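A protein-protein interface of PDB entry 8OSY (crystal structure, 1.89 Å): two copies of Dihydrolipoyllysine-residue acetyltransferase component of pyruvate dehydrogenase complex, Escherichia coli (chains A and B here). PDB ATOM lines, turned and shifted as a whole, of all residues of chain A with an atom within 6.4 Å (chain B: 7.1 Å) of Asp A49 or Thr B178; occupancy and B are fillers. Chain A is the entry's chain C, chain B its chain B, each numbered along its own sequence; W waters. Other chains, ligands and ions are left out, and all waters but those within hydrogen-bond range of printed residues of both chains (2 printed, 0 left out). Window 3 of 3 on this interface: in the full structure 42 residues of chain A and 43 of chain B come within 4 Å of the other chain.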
ATOM      1  N   HIS A  47      13.132 -24.131 -17.537  1.00  0.00           N
ATOM      2  CA  HIS A  47      12.588 -23.446 -18.701  1.00  0.00           C
ATOM      3  C   HIS A  47      12.795 -21.943 -18.554  1.00  0.00           C
ATOM      4  O   HIS A  47      12.731 -21.398 -17.452  1.00  0.00           O
ATOM      5  CB  HIS A  47      11.091 -23.727 -18.847  1.00  0.00           C
ATOM      6  CG  HIS A  47      10.771 -25.080 -19.409  1.00  0.00           C
ATOM      7  ND1 HIS A  47      11.722 -26.066 -19.578  1.00  0.00           N
ATOM      8  CD2 HIS A  47       9.589 -25.631 -19.783  1.00  0.00           C
ATOM      9  CE1 HIS A  47      11.149 -27.148 -20.075  1.00  0.00           C
ATOM     10  NE2 HIS A  47       9.856 -26.909 -20.213  1.00  0.00           N
ATOM     11  N   PHE A  48      12.994 -21.269 -19.677  1.00  0.00           N
ATOM     12  CA  PHE A  48      13.140 -19.822 -19.685  1.00  0.00           C
ATOM     13  C   PHE A  48      12.072 -19.229 -20.592  1.00  0.00           C
ATOM     14  O   PHE A  48      11.603 -19.880 -21.535  1.00  0.00           O
ATOM     15  CB  PHE A  48      14.553 -19.405 -20.141  1.00  0.00           C
ATOM     16  CG  PHE A  48      15.658 -20.014 -19.312  1.00  0.00           C
ATOM     17  CD1 PHE A  48      16.086 -19.405 -18.143  1.00  0.00           C
ATOM     18  CD2 PHE A  48      16.266 -21.208 -19.703  1.00  0.00           C
ATOM     19  CE1 PHE A  48      17.104 -19.969 -17.372  1.00  0.00           C
ATOM     20  CE2 PHE A  48      17.289 -21.783 -18.929  1.00  0.00           C
ATOM     21  CZ  PHE A  48      17.705 -21.160 -17.771  1.00  0.00           C
ATOM     22  N   ASP A  49      11.673 -17.995 -20.287  1.00  0.00           N
ATOM     23  CA  ASP A  49      10.634 -17.320 -21.053  1.00  0.00           C
ATOM     24  C   ASP A  49      10.730 -15.828 -20.769  1.00  0.00           C
ATOM     25  O   ASP A  49      11.453 -15.392 -19.878  1.00  0.00           O
ATOM     26  CB  ASP A  49       9.243 -17.865 -20.707  1.00  0.00           C
ATOM     27  CG  ASP A  49       8.231 -17.672 -21.836  1.00  0.00           C
ATOM     28  OD1 ASP A  49       8.609 -17.178 -22.920  1.00  0.00           O
ATOM     29  OD2 ASP A  49       7.040 -17.983 -21.624  1.00  0.00           O
ATOM     30  N   LYS A  50       9.991 -15.052 -21.558  1.00  0.00           N
ATOM     31  CA  LYS A  50       9.880 -13.608 -21.395  1.00  0.00           C
ATOM     32  C   LYS A  50       8.425 -13.245 -21.600  1.00  0.00           C
ATOM     33  O   LYS A  50       7.793 -13.745 -22.536  1.00  0.00           O
ATOM     34  CB  LYS A  50      10.724 -12.813 -22.409  1.00  0.00           C
ATOM     35  CG  LYS A  50      12.226 -12.886 -22.252  1.00  0.00           C
ATOM     36  CD  LYS A  50      12.872 -11.992 -23.313  1.00  0.00           C
ATOM     37  CE  LYS A  50      14.375 -12.025 -23.238  1.00  0.00           C
ATOM     38  NZ  LYS A  50      15.067 -11.178 -24.270  1.00  0.00           N
ATOM     39  N   THR A  51       7.891 -12.389 -20.732  1.00  0.00           N
ATOM     40  CA  THR A  51       6.498 -11.980 -20.828  1.00  0.00           C
ATOM     41  C   THR A  51       6.409 -10.475 -21.045  1.00  0.00           C
ATOM     42  O   THR A  51       7.151  -9.701 -20.437  1.00  0.00           O
ATOM     43  CB  THR A  51       5.692 -12.394 -19.579  1.00  0.00           C
ATOM     44  OG1 THR A  51       4.356 -11.890 -19.696  1.00  0.00           O
ATOM     45  CG2 THR A  51       6.308 -11.852 -18.325  1.00  0.00           C
ATOM     46  N   THR A 178      19.529 -11.348 -16.071  1.00  0.00           N
ATOM     47  CA  THR A 178      18.564 -11.408 -17.157  1.00  0.00           C
ATOM     48  C   THR A 178      17.765 -12.702 -17.153  1.00  0.00           C
ATOM     49  O   THR A 178      16.717 -12.763 -17.794  1.00  0.00           O
ATOM     50  CB  THR A 178      19.275 -11.283 -18.507  1.00  0.00           C
ATOM     51  OG1 THR A 178      20.334 -12.247 -18.567  1.00  0.00           O
ATOM     52  CG2 THR A 178      19.860  -9.878 -18.668  1.00  0.00           C
ATOM     53  N   HIS A 179      18.263 -13.729 -16.473  1.00  0.00           N
ATOM     54  CA  HIS A 179      17.559 -14.978 -16.203  1.00  0.00           C
ATOM     55  C   HIS A 179      18.329 -15.685 -15.098  1.00  0.00           C
ATOM     56  O   HIS A 179      19.491 -15.371 -14.839  1.00  0.00           O
ATOM     57  CB  HIS A 179      17.477 -15.931 -17.413  1.00  0.00           C
ATOM     58  CG  HIS A 179      16.219 -15.826 -18.217  1.00  0.00           C
ATOM     59  ND1 HIS A 179      16.213 -15.478 -19.550  1.00  0.00           N
ATOM     60  CD2 HIS A 179      14.919 -15.960 -17.859  1.00  0.00           C
ATOM     61  CE1 HIS A 179      14.968 -15.452 -19.992  1.00  0.00           C
ATOM     62  NE2 HIS A 179      14.161 -15.737 -18.984  1.00  0.00           N
ATOM     63  N   LEU A 214       9.514  -9.006 -19.348  1.00  0.00           N
ATOM     64  CA  LEU A 214       9.923  -9.537 -18.060  1.00  0.00           C
ATOM     65  C   LEU A 214      10.439 -10.950 -18.248  1.00  0.00           C
ATOM     66  O   LEU A 214       9.680 -11.815 -18.710  1.00  0.00           O
ATOM     67  CB  LEU A 214       8.753  -9.530 -17.076  1.00  0.00           C
ATOM     68  CG  LEU A 214       9.064 -10.153 -15.714  1.00  0.00           C
ATOM     69  CD1 LEU A 214       9.982  -9.219 -14.904  1.00  0.00           C
ATOM     70  CD2 LEU A 214       7.769 -10.419 -14.953  1.00  0.00           C
ATOM     71  N   PRO A 215      11.708 -11.225 -17.937  1.00  0.00           N
ATOM     72  CA  PRO A 215      12.223 -12.589 -18.076  1.00  0.00           C
ATOM     73  C   PRO A 215      11.866 -13.408 -16.845  1.00  0.00           C
ATOM     74  O   PRO A 215      12.071 -12.968 -15.713  1.00  0.00           O
ATOM     75  CB  PRO A 215      13.738 -12.393 -18.198  1.00  0.00           C
ATOM     76  CG  PRO A 215      14.013 -11.128 -17.456  1.00  0.00           C
ATOM     77  CD  PRO A 215      12.740 -10.285 -17.464  1.00  0.00           C
ATOM     78  N   ILE A 216      11.317 -14.596 -17.083  1.00  0.00           N
ATOM     79  CA  ILE A 216      10.934 -15.529 -16.035  1.00  0.00           C
ATOM     80  C   ILE A 216      11.560 -16.881 -16.350  1.00  0.00           C
ATOM     81  O   ILE A 216      11.916 -17.184 -17.493  1.00  0.00           O
ATOM     82  CB  ILE A 216       9.401 -15.659 -15.906  1.00  0.00           C
ATOM     83  CG1 ILE A 216       8.801 -16.139 -17.230  1.00  0.00           C
ATOM     84  CG2 ILE A 216       8.786 -14.317 -15.450  1.00  0.00           C
ATOM     85  CD1 ILE A 216       7.285 -16.343 -17.195  1.00  0.00           C
ATOM     86  N   SER A 217      11.688 -17.701 -15.312  1.00  0.00           N
ATOM     87  CA  SER A 217      12.250 -19.033 -15.448  1.00  0.00           C
ATOM     88  C   SER A 217      11.515 -20.003 -14.535  1.00  0.00           C
ATOM     89  O   SER A 217      11.009 -19.627 -13.479  1.00  0.00           O
ATOM     90  CB  SER A 217      13.739 -19.037 -15.116  1.00  0.00           C
ATOM     91  OG  SER A 217      13.934 -18.693 -13.756  1.00  0.00           O
ATOM     92  N   LEU A 218      11.468 -21.262 -14.946  1.00  0.00           N
ATOM     93  CA  LEU A 218      10.701 -22.273 -14.224  1.00  0.00           C
ATOM     94  C   LEU A 218      11.580 -23.504 -14.076  1.00  0.00           C
ATOM     95  O   LEU A 218      11.919 -24.148 -15.074  1.00  0.00           O
ATOM     96  CB  LEU A 218       9.404 -22.604 -14.960  1.00  0.00           C
ATOM     97  CG  LEU A 218       8.539 -23.660 -14.256  1.00  0.00           C
ATOM     98  CD1 LEU A 218       7.632 -23.003 -13.224  1.00  0.00           C
ATOM     99  CD2 LEU A 218       7.698 -24.431 -15.289  1.00  0.00           C
ATOM    100  N   ALA A 231       6.547 -26.355 -20.525  1.00  0.00           N
ATOM    101  CA  ALA A 231       6.318 -25.277 -21.478  1.00  0.00           C
ATOM    102  C   ALA A 231       4.882 -24.767 -21.408  1.00  0.00           C
ATOM    103  O   ALA A 231       4.647 -23.555 -21.468  1.00  0.00           O
ATOM    104  CB  ALA A 231       6.652 -25.733 -22.903  1.00  0.00           C
ATOM    105  N   ILE A 234       4.700 -22.539 -18.114  1.00  0.00           N
ATOM    106  CA  ILE A 234       5.308 -21.215 -18.188  1.00  0.00           C
ATOM    107  C   ILE A 234       4.555 -20.349 -19.195  1.00  0.00           C
ATOM    108  O   ILE A 234       4.438 -19.132 -19.016  1.00  0.00           O
ATOM    109  CB  ILE A 234       6.820 -21.319 -18.504  1.00  0.00           C
ATOM    110  CG1 ILE A 234       7.569 -20.041 -18.080  1.00  0.00           C
ATOM    111  CG2 ILE A 234       7.069 -21.664 -19.972  1.00  0.00           C
ATOM    112  CD1 ILE A 234       9.066 -20.259 -17.868  1.00  0.00           C
ATOM    113  N   THR A 235       3.991 -20.964 -20.236  1.00  0.00           N
ATOM    114  CA  THR A 235       3.204 -20.209 -21.208  1.00  0.00           C
ATOM    115  C   THR A 235       1.937 -19.637 -20.578  1.00  0.00           C
ATOM    116  O   THR A 235       1.557 -18.496 -20.869  1.00  0.00           O
ATOM    117  CB  THR A 235       2.861 -21.094 -22.407  1.00  0.00           C
ATOM    118  OG1 THR A 235       4.065 -21.420 -23.115  1.00  0.00           O
ATOM    119  CG2 THR A 235       1.911 -20.388 -23.357  1.00  0.00           C
ATOM    120  N   ASN A 238       2.951 -16.674 -18.522  1.00  0.00           N
ATOM    121  CA  ASN A 238       3.242 -15.630 -19.501  1.00  0.00           C
ATOM    122  C   ASN A 238       1.962 -14.963 -20.001  1.00  0.00           C
ATOM    123  O   ASN A 238       1.790 -13.741 -19.902  1.00  0.00           O
ATOM    124  CB  ASN A 238       4.038 -16.259 -20.653  1.00  0.00           C
ATOM    125  CG  ASN A 238       4.504 -15.251 -21.698  1.00  0.00           C
ATOM    126  OD1 ASN A 238       3.950 -14.165 -21.844  1.00  0.00           O
ATOM    127  ND2 ASN A 238       5.544 -15.632 -22.448  1.00  0.00           N
ATOM    128  N   PHE B  48      23.740 -22.668 -24.671  1.00  0.00           N
ATOM    129  CA  PHE B  48      22.633 -22.013 -25.354  1.00  0.00           C
ATOM    130  C   PHE B  48      23.133 -21.361 -26.640  1.00  0.00           C
ATOM    131  O   PHE B  48      24.276 -20.903 -26.713  1.00  0.00           O
ATOM    132  CB  PHE B  48      21.976 -20.974 -24.447  1.00  0.00           C
ATOM    133  CG  PHE B  48      21.493 -21.552 -23.126  1.00  0.00           C
ATOM    134  CD1 PHE B  48      20.270 -22.215 -23.045  1.00  0.00           C
ATOM    135  CD2 PHE B  48      22.285 -21.473 -21.984  1.00  0.00           C
ATOM    136  CE1 PHE B  48      19.831 -22.776 -21.832  1.00  0.00           C
ATOM    137  CE2 PHE B  48      21.852 -22.022 -20.754  1.00  0.00           C
ATOM    138  CZ  PHE B  48      20.618 -22.676 -20.684  1.00  0.00           C
ATOM    139  N   ASP B  49      22.265 -21.313 -27.648  1.00  0.00           N
ATOM    140  CA  ASP B  49      22.590 -20.682 -28.924  1.00  0.00           C
ATOM    141  C   ASP B  49      21.293 -20.282 -29.619  1.00  0.00           C
ATOM    142  O   ASP B  49      20.194 -20.622 -29.174  1.00  0.00           O
ATOM    143  CB  ASP B  49      23.433 -21.616 -29.801  1.00  0.00           C
ATOM    144  CG  ASP B  49      24.210 -20.882 -30.870  1.00  0.00           C
ATOM    145  OD1 ASP B  49      24.234 -19.628 -30.853  1.00  0.00           O
ATOM    146  OD2 ASP B  49      24.787 -21.572 -31.739  1.00  0.00           O
ATOM    147  N   LYS B  50      21.442 -19.542 -30.721  1.00  0.00           N
ATOM    148  CA  LYS B  50      20.337 -19.104 -31.567  1.00  0.00           C
ATOM    149  C   LYS B  50      20.766 -19.264 -33.021  1.00  0.00           C
ATOM    150  O   LYS B  50      21.852 -18.818 -33.398  1.00  0.00           O
ATOM    151  CB  LYS B  50      19.955 -17.642 -31.290  1.00  0.00           C
ATOM    152  CG  LYS B  50      19.322 -17.349 -29.929  1.00  0.00           C
ATOM    153  CD  LYS B  50      18.894 -15.873 -29.845  1.00  0.00           C
ATOM    154  CE  LYS B  50      17.694 -15.666 -28.925  1.00  0.00           C
ATOM    155  NZ  LYS B  50      17.477 -14.226 -28.591  1.00  0.00           N
ATOM    156  N   LEU B 175       5.019 -25.362 -27.846  1.00  0.00           N
ATOM    157  CA  LEU B 175       4.257 -25.136 -26.629  1.00  0.00           C
ATOM    158  C   LEU B 175       4.759 -23.945 -25.819  1.00  0.00           C
ATOM    159  O   LEU B 175       4.030 -23.463 -24.943  1.00  0.00           O
ATOM    160  CB  LEU B 175       4.280 -26.399 -25.762  1.00  0.00           C
ATOM    161  CG  LEU B 175       3.601 -27.603 -26.434  1.00  0.00           C
ATOM    162  CD1 LEU B 175       3.951 -28.894 -25.709  1.00  0.00           C
ATOM    163  CD2 LEU B 175       2.065 -27.407 -26.478  1.00  0.00           C
ATOM    164  N   GLY B 176       5.972 -23.466 -26.089  1.00  0.00           N
ATOM    165  CA  GLY B 176       6.488 -22.265 -25.472  1.00  0.00           C
ATOM    166  C   GLY B 176       7.959 -22.399 -25.134  1.00  0.00           C
ATOM    167  O   GLY B 176       8.659 -23.263 -25.663  1.00  0.00           O
ATOM    168  N   THR B 177       8.403 -21.508 -24.237  1.00  0.00           N
ATOM    169  CA  THR B 177       9.787 -21.313 -23.791  1.00  0.00           C
ATOM    170  C   THR B 177      10.619 -20.581 -24.836  1.00  0.00           C
ATOM    171  O   THR B 177      10.419 -20.761 -26.038  1.00  0.00           O
ATOM    172  CB  THR B 177      10.516 -22.621 -23.431  1.00  0.00           C
ATOM    173  OG1 THR B 177      10.911 -23.322 -24.619  1.00  0.00           O
ATOM    174  CG2 THR B 177       9.665 -23.528 -22.535  1.00  0.00           C
ATOM    175  N   THR B 178      11.556 -19.753 -24.373  1.00  0.00           N
ATOM    176  CA  THR B 178      12.562 -19.134 -25.226  1.00  0.00           C
ATOM    177  C   THR B 178      13.886 -19.884 -25.209  1.00  0.00           C
ATOM    178  O   THR B 178      14.755 -19.584 -26.022  1.00  0.00           O
ATOM    179  CB  THR B 178      12.813 -17.683 -24.790  1.00  0.00           C
ATOM    180  OG1 THR B 178      13.169 -17.660 -23.399  1.00  0.00           O
ATOM    181  CG2 THR B 178      11.565 -16.852 -24.995  1.00  0.00           C
ATOM    182  N   HIS B 179      14.051 -20.836 -24.296  1.00  0.00           N
ATOM    183  CA  HIS B 179      15.220 -21.680 -24.073  1.00  0.00           C
ATOM    184  C   HIS B 179      14.867 -22.627 -22.940  1.00  0.00           C
ATOM    185  O   HIS B 179      13.983 -22.331 -22.132  1.00  0.00           O
ATOM    186  CB  HIS B 179      16.488 -20.890 -23.689  1.00  0.00           C
ATOM    187  CG  HIS B 179      17.403 -20.598 -24.838  1.00  0.00           C
ATOM    188  ND1 HIS B 179      17.927 -19.345 -25.075  1.00  0.00           N
ATOM    189  CD2 HIS B 179      17.908 -21.407 -25.801  1.00  0.00           C
ATOM    190  CE1 HIS B 179      18.704 -19.390 -26.144  1.00  0.00           C
ATOM    191  NE2 HIS B 179      18.703 -20.628 -26.609  1.00  0.00           N
ATOM    192  N   PHE B 180      15.574 -23.751 -22.867  1.00  0.00           N
ATOM    193  CA  PHE B 180      15.466 -24.582 -21.670  1.00  0.00           C
ATOM    194  C   PHE B 180      16.685 -25.484 -21.576  1.00  0.00           C
ATOM    195  O   PHE B 180      17.469 -25.603 -22.521  1.00  0.00           O
ATOM    196  CB  PHE B 180      14.150 -25.365 -21.638  1.00  0.00           C
ATOM    197  CG  PHE B 180      14.099 -26.572 -22.541  1.00  0.00           C
ATOM    198  CD1 PHE B 180      14.048 -26.432 -23.918  1.00  0.00           C
ATOM    199  CD2 PHE B 180      14.017 -27.846 -21.984  1.00  0.00           C
ATOM    200  CE1 PHE B 180      13.938 -27.551 -24.741  1.00  0.00           C
ATOM    201  CE2 PHE B 180      13.912 -28.983 -22.796  1.00  0.00           C
ATOM    202  CZ  PHE B 180      13.876 -28.832 -24.171  1.00  0.00           C
ATOM    203  N   VAL B 194      15.060 -27.531 -28.188  1.00  0.00           N
ATOM    204  CA  VAL B 194      14.636 -26.572 -29.207  1.00  0.00           C
ATOM    205  C   VAL B 194      13.433 -25.808 -28.675  1.00  0.00           C
ATOM    206  O   VAL B 194      12.410 -26.415 -28.322  1.00  0.00           O
ATOM    207  CB  VAL B 194      14.289 -27.245 -30.549  1.00  0.00           C
ATOM    208  CG1 VAL B 194      13.924 -26.184 -31.593  1.00  0.00           C
ATOM    209  CG2 VAL B 194      15.436 -28.118 -31.031  1.00  0.00           C
ATOM    210  N   SER B 195      13.542 -24.481 -28.637  1.00  0.00           N
ATOM    211  CA  SER B 195      12.489 -23.635 -28.097  1.00  0.00           C
ATOM    212  C   SER B 195      11.861 -22.815 -29.229  1.00  0.00           C
ATOM    213  O   SER B 195      12.084 -23.084 -30.417  1.00  0.00           O
ATOM    214  CB  SER B 195      13.057 -22.773 -26.969  1.00  0.00           C
ATOM    215  OG  SER B 195      13.442 -23.593 -25.876  1.00  0.00           O
ATOM    216  N   LYS B 196      11.071 -21.810 -28.858  1.00  0.00           N
ATOM    217  CA  LYS B 196      10.192 -21.140 -29.813  1.00  0.00           C
ATOM    218  C   LYS B 196      10.955 -20.102 -30.635  1.00  0.00           C
ATOM    219  O   LYS B 196      11.652 -19.244 -30.087  1.00  0.00           O
ATOM    220  CB  LYS B 196       9.006 -20.495 -29.083  1.00  0.00           C
ATOM    221  CG  LYS B 196       9.281 -19.176 -28.376  1.00  0.00           C
ATOM    222  CD  LYS B 196       8.055 -18.626 -27.621  1.00  0.00           C
ATOM    223  CE  LYS B 196       8.476 -17.721 -26.459  1.00  0.00           C
ATOM    224  NZ  LYS B 196       7.387 -17.368 -25.475  1.00  0.00           N
ATOM    225  N   SER B 197      10.830 -20.191 -31.956  1.00  0.00           N
ATOM    226  CA  SER B 197      11.488 -19.233 -32.829  1.00  0.00           C
ATOM    227  C   SER B 197      10.812 -17.867 -32.727  1.00  0.00           C
ATOM    228  O   SER B 197       9.638 -17.749 -32.359  1.00  0.00           O
ATOM    229  CB  SER B 197      11.460 -19.710 -34.280  1.00  0.00           C
ATOM    230  OG  SER B 197      10.149 -19.628 -34.811  1.00  0.00           O
ATOM    231  N   ALA B 198      11.576 -16.824 -33.051  1.00  0.00           N
ATOM    232  CA  ALA B 198      11.053 -15.465 -33.016  1.00  0.00           C
ATOM    233  C   ALA B 198      11.843 -14.572 -33.967  1.00  0.00           C
ATOM    234  O   ALA B 198      13.064 -14.705 -34.074  1.00  0.00           O
ATOM    235  CB  ALA B 198      11.111 -14.890 -31.599  1.00  0.00           C
ATOM    236  N   LEU B 214      16.027 -19.171 -34.158  1.00  0.00           N
ATOM    237  CA  LEU B 214      15.563 -20.359 -33.455  1.00  0.00           C
ATOM    238  C   LEU B 214      16.461 -20.623 -32.261  1.00  0.00           C
ATOM    239  O   LEU B 214      17.653 -20.909 -32.443  1.00  0.00           O
ATOM    240  CB  LEU B 214      15.551 -21.573 -34.388  1.00  0.00           C
ATOM    241  CG  LEU B 214      15.117 -22.875 -33.706  1.00  0.00           C
ATOM    242  CD1 LEU B 214      13.602 -22.907 -33.496  1.00  0.00           C
ATOM    243  CD2 LEU B 214      15.582 -24.103 -34.499  1.00  0.00           C
ATOM    244  N   PRO B 215      15.945 -20.543 -31.036  1.00  0.00           N
ATOM    245  CA  PRO B 215      16.781 -20.821 -29.859  1.00  0.00           C
ATOM    246  C   PRO B 215      16.938 -22.320 -29.661  1.00  0.00           C
ATOM    247  O   PRO B 215      15.962 -23.075 -29.695  1.00  0.00           O
ATOM    248  CB  PRO B 215      16.000 -20.190 -28.706  1.00  0.00           C
ATOM    249  CG  PRO B 215      14.556 -20.136 -29.196  1.00  0.00           C
ATOM    250  CD  PRO B 215      14.549 -20.228 -30.694  1.00  0.00           C
ATOM    251  N   ILE B 216      18.179 -22.749 -29.467  1.00  0.00           N
ATOM    252  CA  ILE B 216      18.477 -24.150 -29.242  1.00  0.00           C
ATOM    253  C   ILE B 216      19.356 -24.231 -28.005  1.00  0.00           C
ATOM    254  O   ILE B 216      20.002 -23.259 -27.605  1.00  0.00           O
ATOM    255  CB  ILE B 216      19.170 -24.818 -30.450  1.00  0.00           C
ATOM    256  CG1 ILE B 216      20.464 -24.078 -30.809  1.00  0.00           C
ATOM    257  CG2 ILE B 216      18.234 -24.859 -31.646  1.00  0.00           C
ATOM    258  CD1 ILE B 216      21.332 -24.837 -31.851  1.00  0.00           C
HETATM  259  O   HOH W   1       8.230 -14.462 -25.133  1.00  0.00           O
HETATM  260  O   HOH W   2       6.253 -19.667 -23.542  1.00  0.00           O
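O of Leu B175 is in hydrogen-bond range of OG1 of Thr A235. The backbone carbonyl oxygen (O) of Phe A48 is in hydrogen-bond range of the backbone NH (N) of Thr B178 (2.8 Å). The side-chain hydroxyl (OG1) of Thr B178 lies within hydrogen-bond range of the backbone NH (N) of Asp A49 (3.5 Å). O of His B179 lies within hydrogen-bond range of N of Phe A48 (2.9 Å). NZ of Lys B196 lies within salt-bridge range of OD1 of Asp A49, 2.8 Å away.
O of Asp B49 sits at hydrogen-bond distance from NE2 of His B179, 3.0 Å away. OG of Ser B195 is in hydrogen-bond range of OG1 of Thr B177 (2.8 Å). The backbone carbonyl oxygen (O) of Leu A218 sits at hydrogen-bond distance from the backbone NH (N) of His A47 (2.7 Å). O of Asp A49 is in hydrogen-bond range of NE2 of His A179 (2.9 Å). The backbone carbonyl oxygen of Asp A49 is in hydrogen-bond range of the backbone NH of Ile A216. The side-chain carboxylate (OD2) of Asp A49 sits at hydrogen-bond distance from the side-chain amide nitrogen (ND2) of Asn A238 (2.9 Å).
Thr B177 touches His A47 (CG2 to CD2, 3.5 Å). His B179 touches His A47. His A47 touches Phe B180 (ND1 to CB, 3.3 Å). CZ of Phe B48 touches CE2 of Phe A48, at 3.9 Å. Phe A48 touches Thr B177. CA of Phe B180 touches CD2 of Phe A48, at 3.99 Å. O of Leu B175 touches O of Ala A231 (3.5 Å). N of Gly B176 touches CB of Ala A231 (3.97 Å). CB of Ala A231 touches CG2 of Thr B177 (3.8 Å). Lys B196 touches Asn A238 (NZ to ND2, 3.9 Å).
Asp A49 touches just these residues of chain B: Thr B178 (3.5 Å) and Lys B196 (2.8 Å). Of chain A, only Phe A48 (2.8 Å) and Asp A49 (3.5 Å) come within 4 Å of Thr B178. Of the printed residues of chain B, Phe A48 touches Phe B48, Thr B177, Thr B178, His B179 and Phe B180. Of the printed residues of chain A, Phe B48 touches Phe A48 (3.9 Å). Of the printed residues of chain A, Phe B180 touches His A47 (3.3 Å) and Phe A48 (3.99 Å). Printed residues of chain B within 4 Å of Asn A238: Lys B196 (3.9 Å). Of the printed residues of chain A, Leu B175 touches Ala A231 and Thr A235. Ser B195 touches none of the printed residues of chain A. Leu B214 touches none of the printed residues of chain A.
Printed residues of chain A that touch a printed residue of chain B: His A47, Phe A48, Asp A49, Ala A231, Thr A235 and Asn A238. Of the 17 printed residues of chain B, 8 touch a printed residue of chain A.
Phe B48 touches its own counterpart, Phe A48. Phe A48 touches Thr B178, but with the chains exchanged Thr A178 does not touch Phe B48 (10.0 Å). Phe A48 touches His B179, but with the chains exchanged His A179 does not touch Phe B48 (8.1 Å). Asp A49 touches Thr B178, but with the chains exchanged Thr A178 does not touch Asp B49 (13.0 Å). 8 positions are printed for both chains.
Water W2 lies within hydrogen-bond range of the side-chain carboxylate (OD2) of Asp A49, the side-chain hydroxyl (OG1) of Thr A235, the backbone NH (N) of Thr B177 and the side-chain amino group (NZ) of Lys B196. Water W1 lies within hydrogen-bond range of O of Lys A50 (2.7 Å) and NZ of Lys B196 (3.0 Å).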
